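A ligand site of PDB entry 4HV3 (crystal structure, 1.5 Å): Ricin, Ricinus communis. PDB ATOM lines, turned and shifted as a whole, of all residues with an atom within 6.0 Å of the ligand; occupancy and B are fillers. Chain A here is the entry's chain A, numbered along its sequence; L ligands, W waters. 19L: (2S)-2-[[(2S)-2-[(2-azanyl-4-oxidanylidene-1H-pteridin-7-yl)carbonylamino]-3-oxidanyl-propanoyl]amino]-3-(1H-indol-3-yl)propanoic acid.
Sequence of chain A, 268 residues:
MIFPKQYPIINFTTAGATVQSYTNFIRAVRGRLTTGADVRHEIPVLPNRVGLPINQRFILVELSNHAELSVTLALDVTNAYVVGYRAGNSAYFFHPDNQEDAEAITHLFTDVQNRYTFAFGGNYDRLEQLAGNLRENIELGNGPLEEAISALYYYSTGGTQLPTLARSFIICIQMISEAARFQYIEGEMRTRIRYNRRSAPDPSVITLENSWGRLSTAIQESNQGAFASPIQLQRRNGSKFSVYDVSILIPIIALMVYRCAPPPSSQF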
ATOM      1  N   ASN A  79      -2.205 -18.650 -28.006  1.00  0.00           N
ATOM      2  CA  ASN A  79      -2.440 -17.457 -28.908  1.00  0.00           C
ATOM      3  C   ASN A  79      -1.785 -16.243 -28.276  1.00  0.00           C
ATOM      4  O   ASN A  79      -1.950 -15.169 -28.897  1.00  0.00           O
ATOM      5  CB  ASN A  79      -3.931 -17.216 -29.137  1.00  0.00           C
ATOM      6  CG  ASN A  79      -4.693 -17.200 -27.792  1.00  0.00           C
ATOM      7  OD1 ASN A  79      -4.131 -16.943 -26.703  1.00  0.00           O
ATOM      8  ND2 ASN A  79      -6.008 -17.500 -27.876  1.00  0.00           N
ATOM      9  N   ALA A  80      -1.080 -16.377 -27.150  1.00  0.00           N
ATOM     10  CA  ALA A  80      -0.444 -15.221 -26.449  1.00  0.00           C
ATOM     11  C   ALA A  80      -1.502 -14.171 -25.950  1.00  0.00           C
ATOM     12  O   ALA A  80      -1.097 -13.123 -25.462  1.00  0.00           O
ATOM     13  CB  ALA A  80       0.620 -14.484 -27.291  1.00  0.00           C
ATOM     14  N   TYR A  81      -2.784 -14.568 -25.869  1.00  0.00           N
ATOM     15  CA  TYR A  81      -3.785 -13.591 -25.372  1.00  0.00           C
ATOM     16  C   TYR A  81      -3.697 -13.407 -23.900  1.00  0.00           C
ATOM     17  O   TYR A  81      -3.419 -14.324 -23.140  1.00  0.00           O
ATOM     18  CB  TYR A  81      -5.202 -14.112 -25.681  1.00  0.00           C
ATOM     19  CG  TYR A  81      -5.748 -13.632 -26.995  1.00  0.00           C
ATOM     20  CD1 TYR A  81      -6.977 -12.960 -27.082  1.00  0.00           C
ATOM     21  CD2 TYR A  81      -5.029 -13.867 -28.204  1.00  0.00           C
ATOM     22  CE1 TYR A  81      -7.453 -12.543 -28.355  1.00  0.00           C
ATOM     23  CE2 TYR A  81      -5.498 -13.445 -29.462  1.00  0.00           C
ATOM     24  CZ  TYR A  81      -6.712 -12.722 -29.541  1.00  0.00           C
ATOM     25  OH  TYR A  81      -7.092 -12.288 -30.826  1.00  0.00           O
ATOM     26  N   VAL A  82      -3.867 -12.125 -23.468  1.00  0.00           N
ATOM     27  CA  VAL A  82      -3.971 -11.893 -22.012  1.00  0.00           C
ATOM     28  C   VAL A  82      -5.378 -12.311 -21.609  1.00  0.00           C
ATOM     29  O   VAL A  82      -6.313 -11.744 -22.126  1.00  0.00           O
ATOM     30  CB  VAL A  82      -3.782 -10.376 -21.794  1.00  0.00           C
ATOM     31  CG1 VAL A  82      -4.052 -10.030 -20.323  1.00  0.00           C
ATOM     32  CG2 VAL A  82      -2.338  -9.971 -22.251  1.00  0.00           C
ATOM     33  N   VAL A  83      -5.489 -13.285 -20.706  1.00  0.00           N
ATOM     34  CA  VAL A  83      -6.849 -13.735 -20.349  1.00  0.00           C
ATOM     35  C   VAL A  83      -7.294 -13.137 -19.033  1.00  0.00           C
ATOM     36  O   VAL A  83      -8.516 -13.247 -18.724  1.00  0.00           O
ATOM     37  CB  VAL A  83      -6.869 -15.326 -20.262  1.00  0.00           C
ATOM     38  CG1 VAL A  83      -6.481 -15.895 -21.653  1.00  0.00           C
ATOM     39  CG2 VAL A  83      -5.997 -15.865 -19.147  1.00  0.00           C
ATOM     40  N   PHE A  94     -11.125 -11.822 -18.329  1.00  0.00           N
ATOM     41  CA  PHE A  94     -12.061 -11.494 -19.388  1.00  0.00           C
ATOM     42  C   PHE A  94     -13.131 -12.618 -19.566  1.00  0.00           C
ATOM     43  O   PHE A  94     -12.869 -13.776 -19.179  1.00  0.00           O
ATOM     44  CB  PHE A  94     -11.431 -11.211 -20.785  1.00  0.00           C
ATOM     45  CG  PHE A  94     -10.470 -10.100 -20.723  1.00  0.00           C
ATOM     46  CD1 PHE A  94     -10.939  -8.805 -20.566  1.00  0.00           C
ATOM     47  CD2 PHE A  94      -9.101 -10.332 -20.874  1.00  0.00           C
ATOM     48  CE1 PHE A  94     -10.031  -7.702 -20.530  1.00  0.00           C
ATOM     49  CE2 PHE A  94      -8.223  -9.239 -20.819  1.00  0.00           C
ATOM     50  CZ  PHE A  94      -8.675  -7.892 -20.681  1.00  0.00           C
ATOM     51  N   ASP A  97     -14.629 -17.227 -23.931  1.00  0.00           N
ATOM     52  CA  ASP A  97     -15.186 -17.505 -25.190  1.00  0.00           C
ATOM     53  C   ASP A  97     -15.933 -18.843 -25.285  1.00  0.00           C
ATOM     54  O   ASP A  97     -16.732 -19.030 -26.203  1.00  0.00           O
ATOM     55  CB  ASP A  97     -14.037 -17.610 -26.197  1.00  0.00           C
ATOM     56  CG  ASP A  97     -13.560 -16.255 -26.715  1.00  0.00           C
ATOM     57  OD1 ASP A  97     -12.627 -16.262 -27.562  1.00  0.00           O
ATOM     58  OD2 ASP A  97     -14.123 -15.206 -26.327  1.00  0.00           O
ATOM     59  N   GLY A 122     -12.281  -9.726 -23.896  1.00  0.00           N
ATOM     60  CA  GLY A 122     -11.063  -8.902 -23.950  1.00  0.00           C
ATOM     61  C   GLY A 122     -10.569  -8.679 -25.380  1.00  0.00           C
ATOM     62  O   GLY A 122      -9.356  -8.259 -25.495  1.00  0.00           O
ATOM     63  N   ASN A 123     -11.327  -8.807 -26.485  1.00  0.00           N
ATOM     64  CA  ASN A 123     -10.883  -8.513 -27.848  1.00  0.00           C
ATOM     65  C   ASN A 123     -10.709  -7.005 -28.029  1.00  0.00           C
ATOM     66  O   ASN A 123     -11.309  -6.203 -27.272  1.00  0.00           O
ATOM     67  CB  ASN A 123     -11.871  -9.085 -28.872  1.00  0.00           C
ATOM     68  CG  ASN A 123     -13.291  -8.573 -28.630  1.00  0.00           C
ATOM     69  OD1 ASN A 123     -13.631  -7.512 -29.189  1.00  0.00           O
ATOM     70  ND2 ASN A 123     -14.108  -9.264 -27.717  1.00  0.00           N
ATOM     71  N   TYR A 124      -9.878  -6.581 -28.981  1.00  0.00           N
ATOM     72  CA  TYR A 124      -9.628  -5.159 -29.156  1.00  0.00           C
ATOM     73  C   TYR A 124     -10.933  -4.375 -29.405  1.00  0.00           C
ATOM     74  O   TYR A 124     -11.051  -3.318 -28.801  1.00  0.00           O
ATOM     75  CB  TYR A 124      -8.742  -4.861 -30.359  1.00  0.00           C
ATOM     76  CG  TYR A 124      -7.257  -5.182 -30.167  1.00  0.00           C
ATOM     77  CD1 TYR A 124      -6.584  -4.853 -28.968  1.00  0.00           C
ATOM     78  CD2 TYR A 124      -6.602  -5.815 -31.230  1.00  0.00           C
ATOM     79  CE1 TYR A 124      -5.224  -5.112 -28.850  1.00  0.00           C
ATOM     80  CE2 TYR A 124      -5.220  -6.110 -31.097  1.00  0.00           C
ATOM     81  CZ  TYR A 124      -4.611  -5.770 -29.918  1.00  0.00           C
ATOM     82  OH  TYR A 124      -3.241  -6.018 -29.848  1.00  0.00           O
ATOM     83  N   ASP A 125     -11.851  -4.927 -30.181  1.00  0.00           N
ATOM     84  CA  ASP A 125     -13.057  -4.078 -30.527  1.00  0.00           C
ATOM     85  C   ASP A 125     -13.821  -3.766 -29.221  1.00  0.00           C
ATOM     86  O   ASP A 125     -14.158  -2.568 -28.954  1.00  0.00           O
ATOM     87  CB  ASP A 125     -13.885  -4.888 -31.447  1.00  0.00           C
ATOM     88  CG  ASP A 125     -15.098  -4.134 -31.980  1.00  0.00           C
ATOM     89  OD1 ASP A 125     -15.220  -2.906 -31.941  1.00  0.00           O
ATOM     90  OD2 ASP A 125     -15.967  -4.844 -32.497  1.00  0.00           O
ATOM     91  N   LEU A 127     -12.648  -3.732 -26.178  1.00  0.00           N
ATOM     92  CA  LEU A 127     -11.882  -2.877 -25.277  1.00  0.00           C
ATOM     93  C   LEU A 127     -11.794  -1.462 -25.801  1.00  0.00           C
ATOM     94  O   LEU A 127     -11.822  -0.555 -24.934  1.00  0.00           O
ATOM     95  CB  LEU A 127     -10.411  -3.422 -25.089  1.00  0.00           C
ATOM     96  CG  LEU A 127     -10.332  -4.749 -24.287  1.00  0.00           C
ATOM     97  CD1 LEU A 127      -8.888  -5.192 -24.235  1.00  0.00           C
ATOM     98  CD2 LEU A 127     -10.835  -4.619 -22.818  1.00  0.00           C
ATOM     99  N   ILE A 173      -1.553  -5.285 -23.877  1.00  0.00           N
ATOM    100  CA  ILE A 173      -1.622  -6.334 -24.916  1.00  0.00           C
ATOM    101  C   ILE A 173      -0.682  -6.000 -26.058  1.00  0.00           C
ATOM    102  O   ILE A 173       0.043  -6.896 -26.535  1.00  0.00           O
ATOM    103  CB  ILE A 173      -3.094  -6.449 -25.410  1.00  0.00           C
ATOM    104  CG1 ILE A 173      -3.951  -6.955 -24.271  1.00  0.00           C
ATOM    105  CG2 ILE A 173      -3.184  -7.208 -26.733  1.00  0.00           C
ATOM    106  CD1 ILE A 173      -5.460  -6.631 -24.614  1.00  0.00           C
ATOM    107  N   SER A 177       1.919  -8.907 -25.717  1.00  0.00           N
ATOM    108  CA  SER A 177       1.474  -9.991 -26.670  1.00  0.00           C
ATOM    109  C   SER A 177       1.822  -9.659 -28.126  1.00  0.00           C
ATOM    110  O   SER A 177       2.364 -10.521 -28.882  1.00  0.00           O
ATOM    111  CB  SER A 177       0.008 -10.226 -26.568  1.00  0.00           C
ATOM    112  OG  SER A 177      -0.268 -10.526 -25.197  1.00  0.00           O
ATOM    113  N   GLU A 178       1.520  -8.429 -28.572  1.00  0.00           N
ATOM    114  CA  GLU A 178       1.785  -8.145 -29.966  1.00  0.00           C
ATOM    115  C   GLU A 178       3.271  -8.006 -30.265  1.00  0.00           C
ATOM    116  O   GLU A 178       3.741  -8.470 -31.343  1.00  0.00           O
ATOM    117  CB  GLU A 178       1.105  -6.842 -30.480  1.00  0.00           C
ATOM    118  CG  GLU A 178      -0.389  -6.855 -30.414  1.00  0.00           C
ATOM    119  CD  GLU A 178      -1.043  -7.779 -31.433  1.00  0.00           C
ATOM    120  OE1 GLU A 178      -0.404  -8.619 -32.103  1.00  0.00           O
ATOM    121  OE2 GLU A 178      -2.313  -7.694 -31.502  1.00  0.00           O
ATOM    122  N   ARG A 181       4.396 -11.515 -30.701  1.00  0.00           N
ATOM    123  CA  ARG A 181       3.983 -12.063 -31.972  1.00  0.00           C
ATOM    124  C   ARG A 181       4.843 -11.539 -33.139  1.00  0.00           C
ATOM    125  O   ARG A 181       5.020 -12.286 -34.125  1.00  0.00           O
ATOM    126  CB  ARG A 181       2.482 -11.787 -32.208  1.00  0.00           C
ATOM    127  CG  ARG A 181       1.576 -12.548 -31.274  1.00  0.00           C
ATOM    128  CD  ARG A 181       0.203 -11.921 -31.531  1.00  0.00           C
ATOM    129  NE  ARG A 181      -0.694 -12.481 -30.488  1.00  0.00           N
ATOM    130  CZ  ARG A 181      -1.577 -11.753 -29.742  1.00  0.00           C
ATOM    131  NH1 ARG A 181      -1.774 -10.434 -30.008  1.00  0.00           N
ATOM    132  NH2 ARG A 181      -2.279 -12.382 -28.824  1.00  0.00           N
ATOM    133  N   GLU A 209      -1.374  -6.290 -36.444  1.00  0.00           N
ATOM    134  CA  GLU A 209      -2.253  -6.772 -35.356  1.00  0.00           C
ATOM    135  C   GLU A 209      -3.568  -7.352 -35.976  1.00  0.00           C
ATOM    136  O   GLU A 209      -4.005  -8.447 -35.587  1.00  0.00           O
ATOM    137  CB  GLU A 209      -2.622  -5.646 -34.411  1.00  0.00           C
ATOM    138  CG  GLU A 209      -1.347  -5.029 -33.730  1.00  0.00           C
ATOM    139  CD  GLU A 209      -1.684  -3.911 -32.832  1.00  0.00           C
ATOM    140  OE1 GLU A 209      -2.830  -3.496 -32.745  1.00  0.00           O
ATOM    141  OE2 GLU A 209      -0.785  -3.422 -32.073  1.00  0.00           O
ATOM    142  N   ASN A 210      -4.131  -6.559 -36.912  1.00  0.00           N
ATOM    143  CA  ASN A 210      -5.422  -6.969 -37.400  1.00  0.00           C
ATOM    144  C   ASN A 210      -5.344  -8.210 -38.251  1.00  0.00           C
ATOM    145  O   ASN A 210      -6.429  -8.841 -38.489  1.00  0.00           O
ATOM    146  CB  ASN A 210      -6.025  -5.874 -38.258  1.00  0.00           C
ATOM    147  CG  ASN A 210      -6.502  -4.647 -37.456  1.00  0.00           C
ATOM    148  OD1 ASN A 210      -6.758  -3.548 -38.141  1.00  0.00           O
ATOM    149  ND2 ASN A 210      -6.643  -4.762 -36.220  1.00  0.00           N
ATOM    150  N   SER A 211      -4.155  -8.575 -38.739  1.00  0.00           N
ATOM    151  CA  SER A 211      -4.009  -9.650 -39.767  1.00  0.00           C
ATOM    152  C   SER A 211      -3.278 -10.853 -39.190  1.00  0.00           C
ATOM    153  O   SER A 211      -2.919 -11.754 -39.985  1.00  0.00           O
ATOM    154  CB  SER A 211      -3.251  -9.181 -40.980  1.00  0.00           C
ATOM    155  OG  SER A 211      -3.875  -7.962 -41.547  1.00  0.00           O
ATOM    156  N   TRP A 212      -3.035 -10.914 -37.891  1.00  0.00           N
ATOM    157  CA  TRP A 212      -2.133 -12.034 -37.412  1.00  0.00           C
ATOM    158  C   TRP A 212      -2.707 -13.392 -37.719  1.00  0.00           C
ATOM    159  O   TRP A 212      -1.978 -14.324 -38.119  1.00  0.00           O
ATOM    160  CB  TRP A 212      -1.949 -11.915 -35.911  1.00  0.00           C
ATOM    161  CG  TRP A 212      -0.994 -12.948 -35.326  1.00  0.00           C
ATOM    162  CD1 TRP A 212       0.302 -13.211 -35.732  1.00  0.00           C
ATOM    163  CD2 TRP A 212      -1.252 -13.778 -34.187  1.00  0.00           C
ATOM    164  NE1 TRP A 212       0.846 -14.152 -34.885  1.00  0.00           N
ATOM    165  CE2 TRP A 212      -0.055 -14.537 -33.954  1.00  0.00           C
ATOM    166  CE3 TRP A 212      -2.390 -13.954 -33.338  1.00  0.00           C
ATOM    167  CZ2 TRP A 212       0.042 -15.435 -32.883  1.00  0.00           C
ATOM    168  CZ3 TRP A 212      -2.298 -14.887 -32.254  1.00  0.00           C
ATOM    169  CH2 TRP A 212      -1.084 -15.613 -32.041  1.00  0.00           C
ATOM    170  N   GLY A 213      -3.982 -13.589 -37.515  1.00  0.00           N
ATOM    171  CA  GLY A 213      -4.580 -14.887 -37.830  1.00  0.00           C
ATOM    172  C   GLY A 213      -4.595 -15.168 -39.319  1.00  0.00           C
ATOM    173  O   GLY A 213      -4.272 -16.346 -39.686  1.00  0.00           O
ATOM    174  N   VAL A 257      -0.144 -18.372 -34.742  1.00  0.00           N
ATOM    175  CA  VAL A 257      -1.156 -19.208 -34.046  1.00  0.00           C
ATOM    176  C   VAL A 257      -1.315 -20.486 -34.897  1.00  0.00           C
ATOM    177  O   VAL A 257      -1.228 -20.436 -36.124  1.00  0.00           O
ATOM    178  CB  VAL A 257      -2.516 -18.388 -33.845  1.00  0.00           C
ATOM    179  CG1 VAL A 257      -3.037 -17.920 -35.221  1.00  0.00           C
ATOM    180  CG2 VAL A 257      -3.567 -19.222 -33.131  1.00  0.00           C
ATOM    181  N   ARG A 259      -2.996 -23.088 -37.055  1.00  0.00           N
ATOM    182  CA  ARG A 259      -4.210 -22.988 -37.929  1.00  0.00           C
ATOM    183  C   ARG A 259      -4.441 -24.286 -38.631  1.00  0.00           C
ATOM    184  O   ARG A 259      -5.537 -24.751 -38.711  1.00  0.00           O
ATOM    185  CB  ARG A 259      -4.115 -21.838 -38.937  1.00  0.00           C
ATOM    186  CG  ARG A 259      -4.196 -20.483 -38.290  1.00  0.00           C
ATOM    187  CD  ARG A 259      -5.649 -20.366 -37.886  1.00  0.00           C
ATOM    188  NE  ARG A 259      -5.993 -19.938 -36.534  1.00  0.00           N
ATOM    189  CZ  ARG A 259      -6.425 -18.737 -36.403  1.00  0.00           C
ATOM    190  NH1 ARG A 259      -6.478 -18.072 -37.537  1.00  0.00           N
ATOM    191  NH2 ARG A 259      -6.829 -18.139 -35.282  1.00  0.00           N
HETATM  192  C   19L L   1      -6.408  -9.865 -25.443  1.00  0.00           C
HETATM  193  N   19L L   1      -6.993  -9.853 -24.203  1.00  0.00           N
HETATM  194  O   19L L   1      -3.355 -10.673 -26.821  1.00  0.00           O
HETATM  195  C1  19L L   1      -4.564 -10.318 -26.676  1.00  0.00           C
HETATM  196  N1  19L L   1      -5.123 -10.325 -25.462  1.00  0.00           N
HETATM  197  C2  19L L   1      -5.220  -9.856 -27.837  1.00  0.00           C
HETATM  198  N2  19L L   1      -7.087  -9.352 -26.442  1.00  0.00           N
HETATM  199  O1  19L L   1      -8.781  -8.327 -30.968  1.00  0.00           O
HETATM  200  C3  19L L   1      -6.568  -9.395 -27.667  1.00  0.00           C
HETATM  201  N3  19L L   1      -7.338  -9.072 -28.704  1.00  0.00           N
HETATM  202  C4  19L L   1      -6.803  -9.115 -29.964  1.00  0.00           C
HETATM  203  N4  19L L   1      -4.704  -9.781 -29.167  1.00  0.00           N
HETATM  204  C5  19L L   1      -5.417  -9.416 -30.206  1.00  0.00           C
HETATM  205  C6  19L L   1      -7.702  -8.852 -31.120  1.00  0.00           C
HETATM  206  N5  19L L   1      -7.351  -9.428 -32.323  1.00  0.00           N
HETATM  207  C7  19L L   1      -8.145  -9.333 -33.500  1.00  0.00           C
HETATM  208  C9  19L L   1      -9.331 -10.320 -33.474  1.00  0.00           C
HETATM  209  O3  19L L   1     -10.174 -10.186 -34.392  1.00  0.00           O
HETATM  210  C8  19L L   1      -7.248  -9.585 -34.743  1.00  0.00           C
HETATM  211  O2  19L L   1      -6.876 -10.975 -34.747  1.00  0.00           O
HETATM  212  N6  19L L   1      -9.517 -11.152 -32.463  1.00  0.00           N
HETATM  213  C10 19L L   1     -10.719 -11.994 -32.458  1.00  0.00           C
HETATM  214  C20 19L L   1     -11.061 -12.106 -30.999  1.00  0.00           C
HETATM  215  O4  19L L   1     -12.270 -12.616 -30.714  1.00  0.00           O
HETATM  216  C11 19L L   1     -10.616 -13.378 -33.152  1.00  0.00           C
HETATM  217  C12 19L L   1      -9.588 -14.307 -32.511  1.00  0.00           C
HETATM  218  C13 19L L   1      -9.700 -14.979 -31.328  1.00  0.00           C
HETATM  219  C15 19L L   1      -8.205 -14.586 -32.994  1.00  0.00           C
HETATM  220  N7  19L L   1      -8.558 -15.684 -30.986  1.00  0.00           N
HETATM  221  C14 19L L   1      -7.632 -15.468 -31.959  1.00  0.00           C
HETATM  222  C16 19L L   1      -7.468 -14.101 -34.088  1.00  0.00           C
HETATM  223  C19 19L L   1      -6.306 -15.883 -32.081  1.00  0.00           C
HETATM  224  C17 19L L   1      -6.152 -14.613 -34.218  1.00  0.00           C
HETATM  225  C18 19L L   1      -5.637 -15.491 -33.224  1.00  0.00           C
HETATM  226  O5  19L L   1     -10.308 -11.795 -30.027  1.00  0.00           O
HETATM  227  O   HOH W   1      -5.185 -11.738 -32.752  1.00  0.00           O
HETATM  228  O   HOH W   2      -3.495  -9.627 -33.077  1.00  0.00           O
HETATM  229  O   HOH W   3      -9.792 -11.599 -25.095  1.00  0.00           O
HETATM  230  O   HOH W   4      -8.373  -6.486 -34.994  1.00  0.00           O
HETATM  231  O   HOH W   5     -11.231  -7.311 -31.941  1.00  0.00           O
HETATM  232  O   HOH W   6     -10.700 -12.545 -27.259  1.00  0.00           O
HETATM  233  O   HOH W   7      -7.369 -18.951 -33.025  1.00  0.00           O
HETATM  234  O   HOH W   8     -11.803 -11.700 -36.072  1.00  0.00           O
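O1 of the ligand is in hydrogen-bond range of N of Tyr 124 (2.9 Å).
The backbone NH of Val 82 sits at hydrogen-bond distance from a nitrogen (N1) of the ligand (3.0 Å).
The side-chain hydroxyl (OH) of Tyr 81 is in hydrogen-bond range of a nitrogen (N6) of the ligand (3.1 Å).
The backbone carbonyl oxygen (O) of Val 82 is in hydrogen-bond range of a nitrogen (N) of the ligand.
O of the ligand sits close to OG of Ser 177 (3.5 Å).
The guanidinium group (NH2) of Arg 181 lies within hydrogen-bond range of an oxygen (O) of the ligand (2.8 Å).
O of Gly 122 is in hydrogen-bond range of N of the ligand, 3.1 Å away.
NH2 of Arg 181 lies within hydrogen-bond range of O of Asn 79.
O of Ile 173 sits at hydrogen-bond distance from N of Glu 178 (2.9 Å).
OG of Ser 177 is in hydrogen-bond range of O of Ala 80, 2.7 Å away.
The backbone NH (N) of Phe 94 is in hydrogen-bond range of the backbone carbonyl oxygen (O) of Val 83 (3.0 Å).
The guanidinium group (NH1) of Arg 181 is in salt-bridge range of the side-chain carboxylate (OE1) of Glu 178, at 3.1 Å.
The backbone NH (N) of Asp 125 lies close to the side-chain amide oxygen (OD1) of Asn 123 (3.3 Å).
The side-chain carboxylate (OE2) of Glu 178 sits at hydrogen-bond distance from the side-chain hydroxyl (OH) of Tyr 124 (2.5 Å).
The side-chain amide oxygen (OD1) of Asn 79 sits at hydrogen-bond distance from the backbone NH (N) of Tyr 81.
O of Ala 80 touches O of the ligand (3.6 Å).
Phe 94 touches the ligand (CE2 to N, 3.7 Å).
Asn 123 touches the ligand (CB to O5, 3.3 Å).
Ile 173 touches the ligand.
Glu 178 touches the ligand (OE2 to C5, 3.8 Å).
Glu 209 touches the ligand (O to C8, 3.5 Å).
O of Asn 210 touches C8 of the ligand, at 3.9 Å.
Trp 212 touches the ligand.
Gly 213 touches the ligand.
Arg 259 touches the ligand.
Hydrophobic or aromatic side chains that line the ligand: Tyr 81, Val 82, Phe 94, Tyr 124, Ile 173 and Trp 212.
Of the 23 residues printed, 16 come within 4 Å of the ligand.
Water W1 lies within hydrogen-bond range of O2 of the ligand and OH of Tyr 81.
Water W5 lies within hydrogen-bond range of an oxygen (O1) of the ligand, the backbone NH of Asp 125 and the backbone NH of Tyr 124.
Water W2 lies within hydrogen-bond range of OE2 of Glu 178 (2.8 Å) and O of Glu 209 (2.8 Å).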
